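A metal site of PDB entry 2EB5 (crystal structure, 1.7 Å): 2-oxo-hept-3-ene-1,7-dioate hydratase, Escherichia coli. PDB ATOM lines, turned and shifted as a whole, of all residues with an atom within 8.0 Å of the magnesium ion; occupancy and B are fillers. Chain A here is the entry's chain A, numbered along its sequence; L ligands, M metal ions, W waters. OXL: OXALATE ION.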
ATOM      1  N   LYS A  61      14.250 -12.704  -4.907  1.00  0.00           N
ATOM      2  CA  LYS A  61      14.822 -11.746  -5.840  1.00  0.00           C
ATOM      3  C   LYS A  61      13.969 -11.707  -7.078  1.00  0.00           C
ATOM      4  O   LYS A  61      13.242 -12.647  -7.374  1.00  0.00           O
ATOM      5  CB  LYS A  61      16.282 -12.085  -6.198  1.00  0.00           C
ATOM      6  CG  LYS A  61      16.527 -13.523  -6.660  1.00  0.00           C
ATOM      7  CD  LYS A  61      16.188 -13.801  -8.158  1.00  0.00           C
ATOM      8  CE  LYS A  61      17.220 -13.327  -9.173  1.00  0.00           C
ATOM      9  NZ  LYS A  61      18.572 -13.962  -9.084  1.00  0.00           N
ATOM     10  N   ILE A  62      14.063 -10.578  -7.777  1.00  0.00           N
ATOM     11  CA  ILE A  62      13.478 -10.401  -9.092  1.00  0.00           C
ATOM     12  C   ILE A  62      14.678 -10.260 -10.029  1.00  0.00           C
ATOM     13  O   ILE A  62      15.619  -9.523  -9.723  1.00  0.00           O
ATOM     14  CB  ILE A  62      12.582  -9.140  -9.139  1.00  0.00           C
ATOM     15  CG1 ILE A  62      11.380  -9.290  -8.191  1.00  0.00           C
ATOM     16  CG2 ILE A  62      12.090  -8.880 -10.550  1.00  0.00           C
ATOM     17  CD1 ILE A  62      11.572  -8.529  -6.870  1.00  0.00           C
ATOM     18  N   GLY A  63      14.660 -10.977 -11.156  1.00  0.00           N
ATOM     19  CA  GLY A  63      15.768 -10.981 -12.073  1.00  0.00           C
ATOM     20  C   GLY A  63      15.334 -10.795 -13.519  1.00  0.00           C
ATOM     21  O   GLY A  63      14.144 -10.636 -13.789  1.00  0.00           O
ATOM     22  N   LEU A  64      16.332 -10.821 -14.424  1.00  0.00           N
ATOM     23  CA  LEU A  64      16.163 -10.582 -15.858  1.00  0.00           C
ATOM     24  C   LEU A  64      15.378  -9.312 -16.129  1.00  0.00           C
ATOM     25  O   LEU A  64      14.602  -9.242 -17.077  1.00  0.00           O
ATOM     26  CB  LEU A  64      15.472 -11.775 -16.546  1.00  0.00           C
ATOM     27  CG  LEU A  64      15.961 -13.201 -16.266  1.00  0.00           C
ATOM     28  CD1 LEU A  64      15.067 -14.209 -16.993  1.00  0.00           C
ATOM     29  CD2 LEU A  64      17.429 -13.389 -16.640  1.00  0.00           C
ATOM     30  N   THR A  65      15.582  -8.315 -15.286  1.00  0.00           N
ATOM     31  CA  THR A  65      14.866  -7.063 -15.381  1.00  0.00           C
ATOM     32  C   THR A  65      15.402  -6.256 -16.561  1.00  0.00           C
ATOM     33  O   THR A  65      14.635  -5.707 -17.359  1.00  0.00           O
ATOM     34  CB  THR A  65      14.981  -6.274 -14.056  1.00  0.00           C
ATOM     35  OG1 THR A  65      16.358  -6.163 -13.676  1.00  0.00           O
ATOM     36  CG2 THR A  65      14.232  -6.995 -12.968  1.00  0.00           C
ATOM     37  N   ASP A  79      12.052 -12.651 -13.932  1.00  0.00           N
ATOM     38  CA  ASP A  79      11.916 -13.927 -13.257  1.00  0.00           C
ATOM     39  C   ASP A  79      11.976 -13.655 -11.748  1.00  0.00           C
ATOM     40  O   ASP A  79      12.146 -12.501 -11.321  1.00  0.00           O
ATOM     41  CB  ASP A  79      12.946 -14.971 -13.712  1.00  0.00           C
ATOM     42  CG  ASP A  79      14.382 -14.645 -13.295  1.00  0.00           C
ATOM     43  OD1 ASP A  79      14.615 -13.614 -12.649  1.00  0.00           O
ATOM     44  OD2 ASP A  79      15.305 -15.459 -13.594  1.00  0.00           O
ATOM     45  N   LEU A  83      15.365 -16.450  -1.779  1.00  0.00           N
ATOM     46  CA  LEU A  83      16.612 -16.249  -1.065  1.00  0.00           C
ATOM     47  C   LEU A  83      16.583 -16.969   0.245  1.00  0.00           C
ATOM     48  O   LEU A  83      15.645 -16.798   1.023  1.00  0.00           O
ATOM     49  CB  LEU A  83      16.888 -14.748  -0.834  1.00  0.00           C
ATOM     50  CG  LEU A  83      17.004 -13.895  -2.121  1.00  0.00           C
ATOM     51  CD1 LEU A  83      17.234 -12.436  -1.788  1.00  0.00           C
ATOM     52  CD2 LEU A  83      18.116 -14.410  -3.001  1.00  0.00           C
ATOM     53  N   ILE A 105      29.123 -11.384 -10.091  1.00  0.00           N
ATOM     54  CA  ILE A 105      28.595 -10.366  -9.156  1.00  0.00           C
ATOM     55  C   ILE A 105      27.806  -9.324  -9.908  1.00  0.00           C
ATOM     56  O   ILE A 105      28.243  -8.880 -10.985  1.00  0.00           O
ATOM     57  CB  ILE A 105      29.767  -9.646  -8.425  1.00  0.00           C
ATOM     58  CG1 ILE A 105      30.460 -10.580  -7.417  1.00  0.00           C
ATOM     59  CG2 ILE A 105      29.303  -8.329  -7.752  1.00  0.00           C
ATOM     60  CD1 ILE A 105      29.718 -10.747  -6.102  1.00  0.00           C
ATOM     61  N   GLU A 106      26.643  -8.960  -9.380  1.00  0.00           N
ATOM     62  CA  GLU A 106      25.857  -7.876  -9.962  1.00  0.00           C
ATOM     63  C   GLU A 106      25.326  -6.942  -8.883  1.00  0.00           C
ATOM     64  O   GLU A 106      25.365  -7.248  -7.687  1.00  0.00           O
ATOM     65  CB  GLU A 106      24.772  -8.445 -10.864  1.00  0.00           C
ATOM     66  CG  GLU A 106      23.739  -9.227 -10.101  1.00  0.00           C
ATOM     67  CD  GLU A 106      22.842 -10.018 -11.006  1.00  0.00           C
ATOM     68  OE1 GLU A 106      23.141 -10.164 -12.204  1.00  0.00           O
ATOM     69  OE2 GLU A 106      21.826 -10.515 -10.507  1.00  0.00           O
ATOM     70  N   VAL A 107      24.858  -5.774  -9.308  1.00  0.00           N
ATOM     71  CA  VAL A 107      24.667  -4.646  -8.417  1.00  0.00           C
ATOM     72  C   VAL A 107      23.181  -4.302  -8.299  1.00  0.00           C
ATOM     73  O   VAL A 107      22.550  -3.967  -9.308  1.00  0.00           O
ATOM     74  CB  VAL A 107      25.457  -3.428  -8.958  1.00  0.00           C
ATOM     75  CG1 VAL A 107      25.176  -2.191  -8.122  1.00  0.00           C
ATOM     76  CG2 VAL A 107      26.953  -3.775  -8.948  1.00  0.00           C
ATOM     77  N   GLU A 108      22.640  -4.344  -7.076  1.00  0.00           N
ATOM     78  CA  GLU A 108      21.197  -4.178  -6.860  1.00  0.00           C
ATOM     79  C   GLU A 108      20.844  -3.281  -5.677  1.00  0.00           C
ATOM     80  O   GLU A 108      21.742  -2.770  -4.965  1.00  0.00           O
ATOM     81  CB  GLU A 108      20.550  -5.584  -6.672  1.00  0.00           C
ATOM     82  CG  GLU A 108      21.202  -6.701  -7.511  1.00  0.00           C
ATOM     83  CD  GLU A 108      20.231  -7.790  -7.908  1.00  0.00           C
ATOM     84  OE1 GLU A 108      19.068  -7.711  -7.485  1.00  0.00           O
ATOM     85  OE2 GLU A 108      20.659  -8.711  -8.653  1.00  0.00           O
ATOM     86  N   ALA A 137      22.638  -3.819  -2.235  1.00  0.00           N
ATOM     87  CA  ALA A 137      22.874  -5.265  -2.166  1.00  0.00           C
ATOM     88  C   ALA A 137      23.562  -5.755  -3.417  1.00  0.00           C
ATOM     89  O   ALA A 137      23.137  -5.400  -4.535  1.00  0.00           O
ATOM     90  CB  ALA A 137      21.558  -6.042  -1.949  1.00  0.00           C
ATOM     91  N   LEU A 138      24.599  -6.593  -3.241  1.00  0.00           N
ATOM     92  CA  LEU A 138      25.183  -7.327  -4.370  1.00  0.00           C
ATOM     93  C   LEU A 138      24.520  -8.676  -4.443  1.00  0.00           C
ATOM     94  O   LEU A 138      24.238  -9.266  -3.400  1.00  0.00           O
ATOM     95  CB  LEU A 138      26.694  -7.535  -4.182  1.00  0.00           C
ATOM     96  CG  LEU A 138      27.480  -6.234  -4.027  1.00  0.00           C
ATOM     97  CD1 LEU A 138      28.995  -6.479  -3.978  1.00  0.00           C
ATOM     98  CD2 LEU A 138      27.144  -5.260  -5.186  1.00  0.00           C
ATOM     99  N   GLU A 139      24.268  -9.166  -5.656  1.00  0.00           N
ATOM    100  CA  GLU A 139      23.898 -10.544  -5.840  1.00  0.00           C
ATOM    101  C   GLU A 139      25.071 -11.290  -6.447  1.00  0.00           C
ATOM    102  O   GLU A 139      25.729 -10.770  -7.358  1.00  0.00           O
ATOM    103  CB  GLU A 139      22.673 -10.700  -6.732  1.00  0.00           C
ATOM    104  CG  GLU A 139      22.115 -12.147  -6.556  1.00  0.00           C
ATOM    105  CD  GLU A 139      20.799 -12.434  -7.262  1.00  0.00           C
ATOM    106  OE1 GLU A 139      20.435 -11.682  -8.209  1.00  0.00           O
ATOM    107  OE2 GLU A 139      20.148 -13.432  -6.873  1.00  0.00           O
ATOM    108  N   LEU A 140      25.352 -12.484  -5.923  1.00  0.00           N
ATOM    109  CA  LEU A 140      26.265 -13.430  -6.511  1.00  0.00           C
ATOM    110  C   LEU A 140      25.384 -14.466  -7.193  1.00  0.00           C
ATOM    111  O   LEU A 140      24.615 -15.180  -6.525  1.00  0.00           O
ATOM    112  CB  LEU A 140      27.101 -14.100  -5.408  1.00  0.00           C
ATOM    113  CG  LEU A 140      28.289 -14.969  -5.797  1.00  0.00           C
ATOM    114  CD1 LEU A 140      29.121 -15.160  -4.538  1.00  0.00           C
ATOM    115  CD2 LEU A 140      27.907 -16.300  -6.377  1.00  0.00           C
ATOM    116  N   ILE A 141      25.407 -14.493  -8.517  1.00  0.00           N
ATOM    117  CA  ILE A 141      24.595 -15.470  -9.265  1.00  0.00           C
ATOM    118  C   ILE A 141      25.494 -16.590  -9.783  1.00  0.00           C
ATOM    119  O   ILE A 141      26.700 -16.435  -9.829  1.00  0.00           O
ATOM    120  CB  ILE A 141      23.836 -14.814 -10.426  1.00  0.00           C
ATOM    121  CG1 ILE A 141      24.812 -14.126 -11.387  1.00  0.00           C
ATOM    122  CG2 ILE A 141      22.792 -13.818  -9.884  1.00  0.00           C
ATOM    123  CD1 ILE A 141      24.189 -13.713 -12.707  1.00  0.00           C
ATOM    124  N   ALA A 166      16.449 -19.256 -10.353  1.00  0.00           N
ATOM    125  CA  ALA A 166      16.729 -17.946 -10.922  1.00  0.00           C
ATOM    126  C   ALA A 166      18.225 -17.549 -10.819  1.00  0.00           C
ATOM    127  O   ALA A 166      18.550 -16.367 -10.764  1.00  0.00           O
ATOM    128  CB  ALA A 166      15.842 -16.900 -10.276  1.00  0.00           C
ATOM    129  N   ALA A 167      19.104 -18.561 -10.818  1.00  0.00           N
ATOM    130  CA  ALA A 167      20.557 -18.371 -10.769  1.00  0.00           C
ATOM    131  C   ALA A 167      21.051 -17.933  -9.395  1.00  0.00           C
ATOM    132  O   ALA A 167      22.204 -17.486  -9.277  1.00  0.00           O
ATOM    133  CB  ALA A 167      21.036 -17.336 -11.837  1.00  0.00           C
ATOM    134  N   ASN A 168      20.195 -18.045  -8.373  1.00  0.00           N
ATOM    135  CA  ASN A 168      20.570 -17.590  -7.021  1.00  0.00           C
ATOM    136  C   ASN A 168      21.798 -18.352  -6.467  1.00  0.00           C
ATOM    137  O   ASN A 168      21.987 -19.552  -6.728  1.00  0.00           O
ATOM    138  CB  ASN A 168      19.429 -17.726  -6.021  1.00  0.00           C
ATOM    139  CG  ASN A 168      18.255 -16.827  -6.327  1.00  0.00           C
ATOM    140  OD1 ASN A 168      18.312 -16.055  -7.280  1.00  0.00           O
ATOM    141  ND2 ASN A 168      17.182 -16.927  -5.539  1.00  0.00           N
ATOM    142  N   GLY A 170      24.293 -16.169  -3.911  1.00  0.00           N
ATOM    143  CA  GLY A 170      24.787 -15.375  -2.796  1.00  0.00           C
ATOM    144  C   GLY A 170      24.167 -13.984  -2.814  1.00  0.00           C
ATOM    145  O   GLY A 170      23.694 -13.540  -3.855  1.00  0.00           O
ATOM    146  N   LEU A 236      15.455  -8.485  -3.197  1.00  0.00           N
ATOM    147  CA  LEU A 236      16.399  -7.886  -4.134  1.00  0.00           C
ATOM    148  C   LEU A 236      15.627  -7.544  -5.399  1.00  0.00           C
ATOM    149  O   LEU A 236      14.947  -8.390  -5.967  1.00  0.00           O
ATOM    150  CB  LEU A 236      17.564  -8.831  -4.480  1.00  0.00           C
ATOM    151  CG  LEU A 236      18.880  -8.572  -3.723  1.00  0.00           C
ATOM    152  CD1 LEU A 236      18.686  -8.816  -2.185  1.00  0.00           C
ATOM    153  CD2 LEU A 236      19.975  -9.472  -4.297  1.00  0.00           C
ATOM    154  N   GLY A 237      15.746  -6.287  -5.827  1.00  0.00           N
ATOM    155  CA  GLY A 237      14.913  -5.805  -6.913  1.00  0.00           C
ATOM    156  C   GLY A 237      15.342  -6.047  -8.358  1.00  0.00           C
ATOM    157  O   GLY A 237      14.521  -5.860  -9.270  1.00  0.00           O
ATOM    158  N   GLY A 238      16.595  -6.463  -8.559  1.00  0.00           N
ATOM    159  CA  GLY A 238      17.152  -6.683  -9.902  1.00  0.00           C
ATOM    160  C   GLY A 238      18.423  -5.845 -10.091  1.00  0.00           C
ATOM    161  O   GLY A 238      18.563  -4.757  -9.494  1.00  0.00           O
ATOM    162  N   SER A 239      19.335  -6.346 -10.914  1.00  0.00           N
ATOM    163  CA  SER A 239      20.628  -5.698 -11.127  1.00  0.00           C
ATOM    164  C   SER A 239      20.539  -4.567 -12.142  1.00  0.00           C
ATOM    165  O   SER A 239      19.885  -4.707 -13.173  1.00  0.00           O
ATOM    166  CB  SER A 239      21.641  -6.699 -11.635  1.00  0.00           C
ATOM    167  OG  SER A 239      22.866  -6.020 -11.858  1.00  0.00           O
ATOM    168  N   PHE A 240      21.180  -3.451 -11.827  1.00  0.00           N
ATOM    169  CA  PHE A 240      21.301  -2.361 -12.808  1.00  0.00           C
ATOM    170  C   PHE A 240      22.673  -2.322 -13.482  1.00  0.00           C
ATOM    171  O   PHE A 240      22.977  -1.356 -14.197  1.00  0.00           O
ATOM    172  CB  PHE A 240      20.833  -0.996 -12.280  1.00  0.00           C
ATOM    173  CG  PHE A 240      21.402  -0.591 -10.932  1.00  0.00           C
ATOM    174  CD1 PHE A 240      22.504   0.270 -10.867  1.00  0.00           C
ATOM    175  CD2 PHE A 240      20.783  -0.979  -9.734  1.00  0.00           C
ATOM    176  CE1 PHE A 240      22.998   0.713  -9.635  1.00  0.00           C
ATOM    177  CE2 PHE A 240      21.268  -0.552  -8.489  1.00  0.00           C
ATOM    178  CZ  PHE A 240      22.366   0.297  -8.435  1.00  0.00           C
ATOM    179  N   THR A 241      23.468  -3.365 -13.250  1.00  0.00           N
ATOM    180  CA  THR A 241      24.654  -3.632 -14.073  1.00  0.00           C
ATOM    181  C   THR A 241      24.624  -5.026 -14.683  1.00  0.00           C
ATOM    182  O   THR A 241      23.920  -5.937 -14.192  1.00  0.00           O
ATOM    183  CB  THR A 241      25.997  -3.536 -13.273  1.00  0.00           C
ATOM    184  OG1 THR A 241      26.034  -4.585 -12.279  1.00  0.00           O
ATOM    185  CG2 THR A 241      26.145  -2.188 -12.589  1.00  0.00           C
ATOM    186  N   PRO A 243      26.334  -8.664 -15.093  1.00  0.00           N
ATOM    187  CA  PRO A 243      27.111  -9.381 -14.059  1.00  0.00           C
ATOM    188  C   PRO A 243      28.548  -9.512 -14.478  1.00  0.00           C
ATOM    189  O   PRO A 243      28.841  -9.515 -15.675  1.00  0.00           O
ATOM    190  CB  PRO A 243      26.448 -10.763 -13.993  1.00  0.00           C
ATOM    191  CG  PRO A 243      25.440 -10.803 -15.064  1.00  0.00           C
ATOM    192  CD  PRO A 243      25.481  -9.563 -15.890  1.00  0.00           C
HETATM  193  C1  OXL L   1      19.103  -9.936 -12.259  1.00  0.00           C
HETATM  194  C2  OXL L   1      19.065 -11.405 -12.061  1.00  0.00           C
HETATM  195  O1  OXL L   1      18.848  -9.461 -13.380  1.00  0.00           O
HETATM  196  O2  OXL L   1      19.311 -11.840 -10.919  1.00  0.00           O
HETATM  197  O3  OXL L   1      19.344  -9.185 -11.291  1.00  0.00           O
HETATM  198  O4  OXL L   1      18.771 -12.163 -13.029  1.00  0.00           O
HETATM  199 MG    MG M   1      19.926 -10.307  -9.578  1.00  0.00          MG
HETATM  200  O   HOH W   1      18.122  -9.971  -8.661  1.00  0.00           O
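OE1 of Glu 108 lies within hydrogen-bond range of N of Gly 238, 3.0 Å away.
The backbone NH (N) of Glu 108 is in hydrogen-bond range of the backbone carbonyl oxygen (O) of Ala 137.
OE2 of Glu 139 is in salt-bridge range of NZ of Lys 61 (2.8 Å).
OD1 of Asn 168 lies close to OE2 of Glu 139 (3.2 Å).
The side-chain amino group (NZ) of Lys 61 is in hydrogen-bond range of the backbone carbonyl oxygen (O) of Ala 166, at 2.9 Å.
The side-chain amide oxygen of Asn 168 is in hydrogen-bond range of the side-chain amino group of Lys 61 (2.8 Å).
The side-chain carboxylate (OE2) of Glu 108 binds the magnesium ion (2.0 Å).
The magnesium ion is bound by OE1 of Glu 139.
The magnesium ion is bound by water W1 (2.1 Å).
OE2 of Glu 106 is bound to the magnesium ion, 2.1 Å away.
The magnesium ion is bound by O2 of the ligand (2.1 Å).
An oxygen (O3) of the ligand is bound to the magnesium ion, at 2.1 Å.
The magnesium ion has six donor atoms within binding distance.
Water W1 lies within hydrogen-bond range of the side-chain carboxylate (OE1) of Glu 108 and the backbone carbonyl oxygen (O) of Ile 62.
Residues that only touch the magnesium ion: Lys 61 (3.9 Å).
Within 4 Å of the magnesium ion: Lys 61, Glu 106, Glu 108 and Glu 139.
The nearest printed residue that does not touch the magnesium ion is Ser 239 (4.2 Å).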
